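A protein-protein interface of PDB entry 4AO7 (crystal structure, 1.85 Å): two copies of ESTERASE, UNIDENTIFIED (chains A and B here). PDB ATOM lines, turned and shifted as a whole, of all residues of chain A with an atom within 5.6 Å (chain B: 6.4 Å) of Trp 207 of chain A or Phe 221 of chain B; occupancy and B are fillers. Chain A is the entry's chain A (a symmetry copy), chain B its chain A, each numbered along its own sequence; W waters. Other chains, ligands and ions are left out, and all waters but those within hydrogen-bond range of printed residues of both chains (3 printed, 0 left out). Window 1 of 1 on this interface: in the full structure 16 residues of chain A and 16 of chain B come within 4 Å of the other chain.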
ATOM      1  N   LEU A 205     -22.932  16.116  12.504  1.00  0.00           N
ATOM      2  CA  LEU A 205     -24.236  15.809  13.116  1.00  0.00           C
ATOM      3  C   LEU A 205     -24.138  15.796  14.641  1.00  0.00           C
ATOM      4  O   LEU A 205     -23.067  15.473  15.259  1.00  0.00           O
ATOM      5  CB  LEU A 205     -24.807  14.462  12.627  1.00  0.00           C
ATOM      6  CG  LEU A 205     -25.338  14.357  11.201  1.00  0.00           C
ATOM      7  CD1 LEU A 205     -25.599  12.869  10.858  1.00  0.00           C
ATOM      8  CD2 LEU A 205     -26.583  15.268  10.992  1.00  0.00           C
ATOM      9  N   GLN A 206     -25.285  16.099  15.256  1.00  0.00           N
ATOM     10  CA  GLN A 206     -25.443  16.011  16.698  1.00  0.00           C
ATOM     11  C   GLN A 206     -26.266  14.815  17.039  1.00  0.00           C
ATOM     12  O   GLN A 206     -27.362  14.669  16.523  1.00  0.00           O
ATOM     13  CB  GLN A 206     -26.096  17.289  17.268  1.00  0.00           C
ATOM     14  CG  GLN A 206     -25.138  18.522  17.326  1.00  0.00           C
ATOM     15  CD  GLN A 206     -23.978  18.369  18.327  1.00  0.00           C
ATOM     16  OE1 GLN A 206     -22.831  18.145  17.940  1.00  0.00           O
ATOM     17  NE2 GLN A 206     -24.285  18.477  19.626  1.00  0.00           N
ATOM     18  N   TRP A 207     -25.727  13.964  17.921  1.00  0.00           N
ATOM     19  CA  TRP A 207     -26.364  12.700  18.286  1.00  0.00           C
ATOM     20  C   TRP A 207     -27.808  12.894  18.756  1.00  0.00           C
ATOM     21  O   TRP A 207     -28.735  12.212  18.256  1.00  0.00           O
ATOM     22  CB  TRP A 207     -25.535  11.985  19.360  1.00  0.00           C
ATOM     23  CG  TRP A 207     -25.976  10.567  19.583  1.00  0.00           C
ATOM     24  CD1 TRP A 207     -26.959  10.131  20.425  1.00  0.00           C
ATOM     25  CD2 TRP A 207     -25.424   9.401  18.965  1.00  0.00           C
ATOM     26  NE1 TRP A 207     -27.068   8.753  20.353  1.00  0.00           N
ATOM     27  CE2 TRP A 207     -26.141   8.283  19.459  1.00  0.00           C
ATOM     28  CE3 TRP A 207     -24.401   9.195  18.033  1.00  0.00           C
ATOM     29  CZ2 TRP A 207     -25.856   6.964  19.051  1.00  0.00           C
ATOM     30  CZ3 TRP A 207     -24.115   7.889  17.622  1.00  0.00           C
ATOM     31  CH2 TRP A 207     -24.846   6.795  18.131  1.00  0.00           C
ATOM     32  N   ASP A 208     -27.983  13.841  19.671  1.00  0.00           N
ATOM     33  CA  ASP A 208     -29.268  14.096  20.347  1.00  0.00           C
ATOM     34  C   ASP A 208     -30.016  15.312  19.760  1.00  0.00           C
ATOM     35  O   ASP A 208     -30.854  15.929  20.448  1.00  0.00           O
ATOM     36  CB  ASP A 208     -28.995  14.285  21.846  1.00  0.00           C
ATOM     37  CG  ASP A 208     -28.145  13.153  22.435  1.00  0.00           C
ATOM     38  OD1 ASP A 208     -28.730  12.107  22.775  1.00  0.00           O
ATOM     39  OD2 ASP A 208     -26.896  13.303  22.575  1.00  0.00           O
ATOM     40  N   ASP A 209     -29.709  15.645  18.491  1.00  0.00           N
ATOM     41  CA  ASP A 209     -30.379  16.728  17.753  1.00  0.00           C
ATOM     42  C   ASP A 209     -31.900  16.535  17.747  1.00  0.00           C
ATOM     43  O   ASP A 209     -32.425  15.567  17.193  1.00  0.00           O
ATOM     44  CB  ASP A 209     -29.830  16.846  16.326  1.00  0.00           C
ATOM     45  CG  ASP A 209     -30.203  18.146  15.643  1.00  0.00           C
ATOM     46  OD1 ASP A 209     -31.375  18.593  15.762  1.00  0.00           O
ATOM     47  OD2 ASP A 209     -29.324  18.745  14.950  1.00  0.00           O
ATOM     48  N   LEU A 214     -30.834  11.676  14.021  1.00  0.00           N
ATOM     49  CA  LEU A 214     -29.559  11.123  13.607  1.00  0.00           C
ATOM     50  C   LEU A 214     -29.749  10.244  12.374  1.00  0.00           C
ATOM     51  O   LEU A 214     -29.018  10.375  11.416  1.00  0.00           O
ATOM     52  CB  LEU A 214     -28.956  10.355  14.750  1.00  0.00           C
ATOM     53  CG  LEU A 214     -27.620   9.685  14.452  1.00  0.00           C
ATOM     54  CD1 LEU A 214     -26.575  10.702  14.091  1.00  0.00           C
ATOM     55  CD2 LEU A 214     -27.230   8.878  15.690  1.00  0.00           C
ATOM     56  N   VAL A 233     -19.670  13.066  14.341  1.00  0.00           N
ATOM     57  CA  VAL A 233     -20.865  13.098  15.202  1.00  0.00           C
ATOM     58  C   VAL A 233     -20.464  13.313  16.625  1.00  0.00           C
ATOM     59  O   VAL A 233     -19.574  12.627  17.133  1.00  0.00           O
ATOM     60  CB  VAL A 233     -21.709  11.808  15.113  1.00  0.00           C
ATOM     61  CG1 VAL A 233     -23.092  12.016  15.799  1.00  0.00           C
ATOM     62  CG2 VAL A 233     -21.917  11.389  13.657  1.00  0.00           C
ATOM     63  N   ASN A 234     -21.127  14.269  17.295  1.00  0.00           N
ATOM     64  CA  ASN A 234     -20.855  14.560  18.675  1.00  0.00           C
ATOM     65  C   ASN A 234     -22.139  14.474  19.492  1.00  0.00           C
ATOM     66  O   ASN A 234     -23.216  14.660  18.929  1.00  0.00           O
ATOM     67  CB  ASN A 234     -20.279  15.951  18.808  1.00  0.00           C
ATOM     68  CG  ASN A 234     -18.918  16.057  18.195  1.00  0.00           C
ATOM     69  OD1 ASN A 234     -17.949  15.571  18.758  1.00  0.00           O
ATOM     70  ND2 ASN A 234     -18.832  16.734  17.058  1.00  0.00           N
ATOM     71  N   PRO A 235     -22.019  14.228  20.796  1.00  0.00           N
ATOM     72  CA  PRO A 235     -23.209  14.139  21.650  1.00  0.00           C
ATOM     73  C   PRO A 235     -23.878  15.499  21.792  1.00  0.00           C
ATOM     74  O   PRO A 235     -23.239  16.542  21.608  1.00  0.00           O
ATOM     75  CB  PRO A 235     -22.651  13.709  23.014  1.00  0.00           C
ATOM     76  CG  PRO A 235     -21.320  13.142  22.719  1.00  0.00           C
ATOM     77  CD  PRO A 235     -20.803  13.821  21.532  1.00  0.00           C
ATOM     78  N   GLY A 236     -25.162  15.477  22.111  1.00  0.00           N
ATOM     79  CA  GLY A 236     -25.844  16.712  22.426  1.00  0.00           C
ATOM     80  C   GLY A 236     -26.900  17.160  21.465  1.00  0.00           C
ATOM     81  O   GLY A 236     -27.192  16.538  20.422  1.00  0.00           O
ATOM     82  N   MET B 180     -15.762  -1.621  15.291  1.00  0.00           N
ATOM     83  CA  MET B 180     -16.283  -2.634  16.184  1.00  0.00           C
ATOM     84  C   MET B 180     -17.654  -2.186  16.629  1.00  0.00           C
ATOM     85  O   MET B 180     -17.934  -0.979  16.742  1.00  0.00           O
ATOM     86  CB  MET B 180     -15.348  -2.866  17.395  1.00  0.00           C
ATOM     87  CG  MET B 180     -15.718  -4.058  18.302  1.00  0.00           C
ATOM     88  SD  MET B 180     -16.236  -5.597  17.483  1.00  0.00           S
ATOM     89  CE  MET B 180     -14.907  -5.883  16.326  1.00  0.00           C
ATOM     90  N   VAL B 182     -21.667  -3.945  18.453  1.00  0.00           N
ATOM     91  CA  VAL B 182     -22.280  -4.766  19.498  1.00  0.00           C
ATOM     92  C   VAL B 182     -22.509  -6.207  19.049  1.00  0.00           C
ATOM     93  O   VAL B 182     -22.865  -7.051  19.860  1.00  0.00           O
ATOM     94  CB  VAL B 182     -23.633  -4.174  19.974  1.00  0.00           C
ATOM     95  CG1 VAL B 182     -23.433  -2.735  20.505  1.00  0.00           C
ATOM     96  CG2 VAL B 182     -24.660  -4.201  18.847  1.00  0.00           C
ATOM     97  N   VAL B 201     -12.847   9.927  24.198  1.00  0.00           N
ATOM     98  CA  VAL B 201     -12.799   8.922  23.180  1.00  0.00           C
ATOM     99  C   VAL B 201     -13.007   9.512  21.768  1.00  0.00           C
ATOM    100  O   VAL B 201     -13.903  10.330  21.515  1.00  0.00           O
ATOM    101  CB  VAL B 201     -13.886   7.822  23.396  1.00  0.00           C
ATOM    102  CG1 VAL B 201     -13.869   6.815  22.233  1.00  0.00           C
ATOM    103  CG2 VAL B 201     -13.707   7.105  24.758  1.00  0.00           C
ATOM    104  N   ARG B 202     -12.171   9.074  20.845  1.00  0.00           N
ATOM    105  CA  ARG B 202     -12.460   9.224  19.431  1.00  0.00           C
ATOM    106  C   ARG B 202     -12.711   7.834  18.914  1.00  0.00           C
ATOM    107  O   ARG B 202     -11.920   6.946  19.147  1.00  0.00           O
ATOM    108  CB  ARG B 202     -11.325   9.880  18.637  1.00  0.00           C
ATOM    109  CG  ARG B 202     -11.615   9.898  17.122  1.00  0.00           C
ATOM    110  CD  ARG B 202     -10.597  10.623  16.278  1.00  0.00           C
ATOM    111  NE  ARG B 202     -10.550  12.067  16.537  1.00  0.00           N
ATOM    112  CZ  ARG B 202      -9.775  12.916  15.872  1.00  0.00           C
ATOM    113  NH1 ARG B 202      -8.990  12.479  14.874  1.00  0.00           N
ATOM    114  NH2 ARG B 202      -9.799  14.215  16.180  1.00  0.00           N
ATOM    115  N   TYR B 203     -13.809   7.686  18.193  1.00  0.00           N
ATOM    116  CA  TYR B 203     -14.261   6.412  17.685  1.00  0.00           C
ATOM    117  C   TYR B 203     -14.304   6.505  16.159  1.00  0.00           C
ATOM    118  O   TYR B 203     -14.828   7.482  15.606  1.00  0.00           O
ATOM    119  CB  TYR B 203     -15.638   6.107  18.276  1.00  0.00           C
ATOM    120  CG  TYR B 203     -15.949   4.652  18.341  1.00  0.00           C
ATOM    121  CD1 TYR B 203     -16.509   3.981  17.263  1.00  0.00           C
ATOM    122  CD2 TYR B 203     -15.622   3.926  19.474  1.00  0.00           C
ATOM    123  CE1 TYR B 203     -16.800   2.639  17.347  1.00  0.00           C
ATOM    124  CE2 TYR B 203     -15.895   2.607  19.567  1.00  0.00           C
ATOM    125  CZ  TYR B 203     -16.467   1.951  18.507  1.00  0.00           C
ATOM    126  OH  TYR B 203     -16.678   0.597  18.642  1.00  0.00           O
ATOM    127  N   LEU B 205     -15.520   4.646  12.530  1.00  0.00           N
ATOM    128  CA  LEU B 205     -16.285   3.616  11.806  1.00  0.00           C
ATOM    129  C   LEU B 205     -16.139   3.785  10.294  1.00  0.00           C
ATOM    130  O   LEU B 205     -15.949   4.924   9.745  1.00  0.00           O
ATOM    131  CB  LEU B 205     -17.780   3.627  12.182  1.00  0.00           C
ATOM    132  CG  LEU B 205     -18.202   3.117  13.557  1.00  0.00           C
ATOM    133  CD1 LEU B 205     -19.688   3.475  13.805  1.00  0.00           C
ATOM    134  CD2 LEU B 205     -17.896   1.598  13.714  1.00  0.00           C
ATOM    135  N   SER B 216     -24.594  -1.407  14.101  1.00  0.00           N
ATOM    136  CA  SER B 216     -23.995  -2.080  15.263  1.00  0.00           C
ATOM    137  C   SER B 216     -22.875  -1.228  15.874  1.00  0.00           C
ATOM    138  O   SER B 216     -22.699  -1.188  17.091  1.00  0.00           O
ATOM    139  CB  SER B 216     -23.461  -3.454  14.839  1.00  0.00           C
ATOM    140  OG  SER B 216     -22.762  -4.118  15.877  1.00  0.00           O
ATOM    141  N   GLY B 217     -22.121  -0.545  15.018  1.00  0.00           N
ATOM    142  CA  GLY B 217     -21.064   0.352  15.453  1.00  0.00           C
ATOM    143  C   GLY B 217     -21.649   1.594  16.113  1.00  0.00           C
ATOM    144  O   GLY B 217     -21.176   2.008  17.166  1.00  0.00           O
ATOM    145  N   LEU B 218     -22.685   2.167  15.512  1.00  0.00           N
ATOM    146  CA  LEU B 218     -23.376   3.306  16.128  1.00  0.00           C
ATOM    147  C   LEU B 218     -23.926   2.940  17.500  1.00  0.00           C
ATOM    148  O   LEU B 218     -23.789   3.691  18.475  1.00  0.00           O
ATOM    149  CB  LEU B 218     -24.506   3.807  15.239  1.00  0.00           C
ATOM    150  CG  LEU B 218     -24.040   4.525  13.976  1.00  0.00           C
ATOM    151  CD1 LEU B 218     -25.143   4.606  12.972  1.00  0.00           C
ATOM    152  CD2 LEU B 218     -23.554   5.931  14.327  1.00  0.00           C
ATOM    153  N   GLU B 219     -24.523   1.764  17.596  1.00  0.00           N
ATOM    154  CA  GLU B 219     -25.089   1.364  18.851  1.00  0.00           C
ATOM    155  C   GLU B 219     -24.016   1.325  19.959  1.00  0.00           C
ATOM    156  O   GLU B 219     -24.246   1.828  21.047  1.00  0.00           O
ATOM    157  CB  GLU B 219     -25.808   0.029  18.706  1.00  0.00           C
ATOM    158  CG  GLU B 219     -26.418  -0.428  19.982  1.00  0.00           C
ATOM    159  CD  GLU B 219     -27.393  -1.582  19.820  1.00  0.00           C
ATOM    160  OE1 GLU B 219     -27.754  -1.945  18.674  1.00  0.00           O
ATOM    161  OE2 GLU B 219     -27.767  -2.120  20.867  1.00  0.00           O
ATOM    162  N   LEU B 220     -22.837   0.775  19.677  1.00  0.00           N
ATOM    163  CA  LEU B 220     -21.804   0.704  20.697  1.00  0.00           C
ATOM    164  C   LEU B 220     -21.284   2.104  21.062  1.00  0.00           C
ATOM    165  O   LEU B 220     -21.120   2.410  22.216  1.00  0.00           O
ATOM    166  CB  LEU B 220     -20.663  -0.205  20.264  1.00  0.00           C
ATOM    167  CG  LEU B 220     -19.542  -0.470  21.286  1.00  0.00           C
ATOM    168  CD1 LEU B 220     -20.066  -0.797  22.661  1.00  0.00           C
ATOM    169  CD2 LEU B 220     -18.577  -1.574  20.793  1.00  0.00           C
ATOM    170  N   PHE B 221     -21.063   2.962  20.071  1.00  0.00           N
ATOM    171  CA  PHE B 221     -20.642   4.332  20.339  1.00  0.00           C
ATOM    172  C   PHE B 221     -21.631   5.042  21.279  1.00  0.00           C
ATOM    173  O   PHE B 221     -21.230   5.738  22.221  1.00  0.00           O
ATOM    174  CB  PHE B 221     -20.508   5.109  19.028  1.00  0.00           C
ATOM    175  CG  PHE B 221     -20.118   6.538  19.232  1.00  0.00           C
ATOM    176  CD1 PHE B 221     -18.800   6.886  19.424  1.00  0.00           C
ATOM    177  CD2 PHE B 221     -21.093   7.540  19.282  1.00  0.00           C
ATOM    178  CE1 PHE B 221     -18.449   8.192  19.659  1.00  0.00           C
ATOM    179  CE2 PHE B 221     -20.727   8.873  19.486  1.00  0.00           C
ATOM    180  CZ  PHE B 221     -19.413   9.182  19.681  1.00  0.00           C
ATOM    181  N   GLY B 222     -22.929   4.843  21.019  1.00  0.00           N
ATOM    182  CA  GLY B 222     -23.980   5.432  21.839  1.00  0.00           C
ATOM    183  C   GLY B 222     -23.910   5.049  23.302  1.00  0.00           C
ATOM    184  O   GLY B 222     -24.311   5.832  24.166  1.00  0.00           O
ATOM    185  N   LYS B 223     -23.468   3.822  23.564  1.00  0.00           N
ATOM    186  CA  LYS B 223     -23.432   3.238  24.908  1.00  0.00           C
ATOM    187  C   LYS B 223     -22.219   3.685  25.708  1.00  0.00           C
ATOM    188  O   LYS B 223     -22.208   3.563  26.919  1.00  0.00           O
ATOM    189  CB  LYS B 223     -23.491   1.700  24.817  1.00  0.00           C
ATOM    190  CG  LYS B 223     -24.781   1.199  24.164  1.00  0.00           C
ATOM    191  CD  LYS B 223     -24.929  -0.308  24.153  1.00  0.00           C
ATOM    192  CE  LYS B 223     -26.312  -0.694  23.588  1.00  0.00           C
ATOM    193  NZ  LYS B 223     -27.436  -0.382  24.521  1.00  0.00           N
ATOM    194  N   LEU B 224     -21.203   4.245  25.046  1.00  0.00           N
ATOM    195  CA  LEU B 224     -20.047   4.777  25.763  1.00  0.00           C
ATOM    196  C   LEU B 224     -20.493   5.849  26.770  1.00  0.00           C
ATOM    197  O   LEU B 224     -21.259   6.757  26.428  1.00  0.00           O
ATOM    198  CB  LEU B 224     -19.023   5.384  24.775  1.00  0.00           C
ATOM    199  CG  LEU B 224     -18.316   4.400  23.852  1.00  0.00           C
ATOM    200  CD1 LEU B 224     -17.500   5.182  22.781  1.00  0.00           C
ATOM    201  CD2 LEU B 224     -17.402   3.453  24.613  1.00  0.00           C
ATOM    202  N   GLY B 225     -19.985   5.753  27.997  1.00  0.00           N
ATOM    203  CA  GLY B 225     -20.466   6.589  29.094  1.00  0.00           C
ATOM    204  C   GLY B 225     -20.051   8.037  28.984  1.00  0.00           C
ATOM    205  O   GLY B 225     -20.817   8.935  29.333  1.00  0.00           O
ATOM    206  N   THR B 226     -18.838   8.261  28.478  1.00  0.00           N
ATOM    207  CA  THR B 226     -18.267   9.599  28.393  1.00  0.00           C
ATOM    208  C   THR B 226     -19.073  10.548  27.531  1.00  0.00           C
ATOM    209  O   THR B 226     -19.638  10.166  26.499  1.00  0.00           O
ATOM    210  CB  THR B 226     -16.819   9.539  27.852  1.00  0.00           C
ATOM    211  OG1 THR B 226     -16.234  10.851  27.845  1.00  0.00           O
ATOM    212  CG2 THR B 226     -16.780   8.910  26.461  1.00  0.00           C
ATOM    213  N   LYS B 229     -16.947  12.203  23.814  1.00  0.00           N
ATOM    214  CA  LYS B 229     -16.711  11.199  22.756  1.00  0.00           C
ATOM    215  C   LYS B 229     -17.052  11.821  21.418  1.00  0.00           C
ATOM    216  O   LYS B 229     -17.986  12.627  21.330  1.00  0.00           O
ATOM    217  CB  LYS B 229     -17.526   9.938  22.991  1.00  0.00           C
ATOM    218  CG  LYS B 229     -19.028  10.152  23.114  1.00  0.00           C
ATOM    219  CD  LYS B 229     -19.745   8.877  23.353  1.00  0.00           C
ATOM    220  CE  LYS B 229     -21.236   9.105  23.578  1.00  0.00           C
ATOM    221  NZ  LYS B 229     -22.030   7.854  23.901  1.00  0.00           N
ATOM    222  N   THR B 230     -16.269  11.515  20.385  1.00  0.00           N
ATOM    223  CA  THR B 230     -16.585  11.954  19.029  1.00  0.00           C
ATOM    224  C   THR B 230     -16.450  10.755  18.092  1.00  0.00           C
ATOM    225  O   THR B 230     -15.637   9.860  18.347  1.00  0.00           O
ATOM    226  CB  THR B 230     -15.708  13.162  18.565  1.00  0.00           C
ATOM    227  OG1 THR B 230     -16.259  13.713  17.375  1.00  0.00           O
ATOM    228  CG2 THR B 230     -14.315  12.732  18.229  1.00  0.00           C
ATOM    229  N   LEU B 231     -17.339  10.688  17.094  1.00  0.00           N
ATOM    230  CA  LEU B 231     -17.383   9.581  16.136  1.00  0.00           C
ATOM    231  C   LEU B 231     -16.990  10.146  14.786  1.00  0.00           C
ATOM    232  O   LEU B 231     -17.560  11.161  14.338  1.00  0.00           O
ATOM    233  CB  LEU B 231     -18.785   8.973  16.039  1.00  0.00           C
ATOM    234  CG  LEU B 231     -18.967   7.923  14.933  1.00  0.00           C
ATOM    235  CD1 LEU B 231     -18.228   6.633  15.230  1.00  0.00           C
ATOM    236  CD2 LEU B 231     -20.480   7.567  14.686  1.00  0.00           C
ATOM    237  N   HIS B 232     -16.019   9.507  14.123  1.00  0.00           N
ATOM    238  CA  HIS B 232     -15.671   9.873  12.736  1.00  0.00           C
ATOM    239  C   HIS B 232     -16.025   8.710  11.823  1.00  0.00           C
ATOM    240  O   HIS B 232     -15.560   7.597  12.075  1.00  0.00           O
ATOM    241  CB  HIS B 232     -14.189  10.126  12.586  1.00  0.00           C
ATOM    242  CG  HIS B 232     -13.720  11.407  13.206  1.00  0.00           C
ATOM    243  ND1 HIS B 232     -12.485  11.958  12.935  1.00  0.00           N
ATOM    244  CD2 HIS B 232     -14.308  12.226  14.117  1.00  0.00           C
ATOM    245  CE1 HIS B 232     -12.336  13.062  13.650  1.00  0.00           C
ATOM    246  NE2 HIS B 232     -13.426  13.236  14.386  1.00  0.00           N
HETATM  247  O   HOH W   1     -26.917   7.267  23.463  1.00  0.00           O
HETATM  248  O   HOH W   2     -24.224   9.036  22.359  1.00  0.00           O
HETATM  249  O   HOH W   3     -17.574  15.334  21.550  1.00  0.00           O
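The side-chain hydroxyl of Thr 230 of chain B lies within hydrogen-bond range of the backbone carbonyl oxygen of Val 233 of chain A (3.5 Å). OD1 of Asn 234 of chain A lies within hydrogen-bond range of OG1 of Thr 230 of chain B (2.9 Å). The backbone carbonyl oxygen (O) of Leu 231 of chain B lies within hydrogen-bond range of the backbone NH (N) of Val 233 of chain A.
O of Val 201 of chain B sits at hydrogen-bond distance from N of Thr 230 of chain B (2.9 Å). O of Thr 230 of chain B is in hydrogen-bond range of N of Tyr 203 of chain B (2.8 Å). The backbone carbonyl oxygen of Phe 221 of chain B lies within hydrogen-bond range of the side-chain amino group of Lys 229 of chain B, at 2.8 Å. The backbone carbonyl oxygen (O) of Leu 224 of chain B is in hydrogen-bond range of the side-chain amino group (NZ) of Lys 229 of chain B (2.9 Å). The backbone carbonyl oxygen (O) of Leu 205 of chain A is in hydrogen-bond range of the backbone NH (N) of Asn 234 of chain A (3.1 Å). NE2 of Gln 206 of chain A is in hydrogen-bond range of O of Pro 235 of chain A (3.0 Å).
Among the printed residues, pairs that only touch across the chains: Trp 207 of chain A with Leu 218 of chain B (3.3 Å), Trp 207 of chain A with Phe 221 of chain B (3.5 Å), Trp 207 of chain A with Gly 222 of chain B (3.7 Å), Asn 234 of chain A with Lys 229 of chain B (3.9 Å) and Pro 235 of chain A with Lys 229 of chain B (3.1 Å).
Of chain B, only Leu 218, Phe 221 and Gly 222 come within 4 Å of Trp 207 of chain A. Of the printed residues of chain A, Leu 218 of chain B touches Trp 207. Phe 221 of chain B touches just one residue of chain A: Trp 207. Of the printed residues of chain A, Thr 230 of chain B touches Val 233 and Asn 234. The nearest printed residue of chain A that does not touch Gly 222 of chain B is Leu 214 of chain A (7.8 Å).
Of the 10 printed residues of chain A, 4 touch a printed residue of chain B. Hydrophobic or aromatic side chains of chain A within 4 Å of the printed part of chain B: Trp 207 and Pro 235. Of the 21 printed residues of chain B, 6 touch a printed residue of chain A. Hydrophobic or aromatic side chains of chain B that line the printed part of chain A: Leu 218, Phe 221 and Leu 231. Along chain B the printed residues that touch a printed residue of chain A span positions 218 to 231. Among the printed residues, 8 pairs touch across the chains.
Position printed for both chains: 205.
Water W3 bridges the backbone carbonyl oxygen (O) of Lys 229 of chain B and the side-chain amide oxygen (OD1) of Asn 234 of chain A. Water W2 lies within hydrogen-bond range of NZ of Lys 229 of chain B and NE1 of Trp 207 of chain A. Water W1 bridges O of Gly 222 of chain B and NE1 of Trp 207 of chain A.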
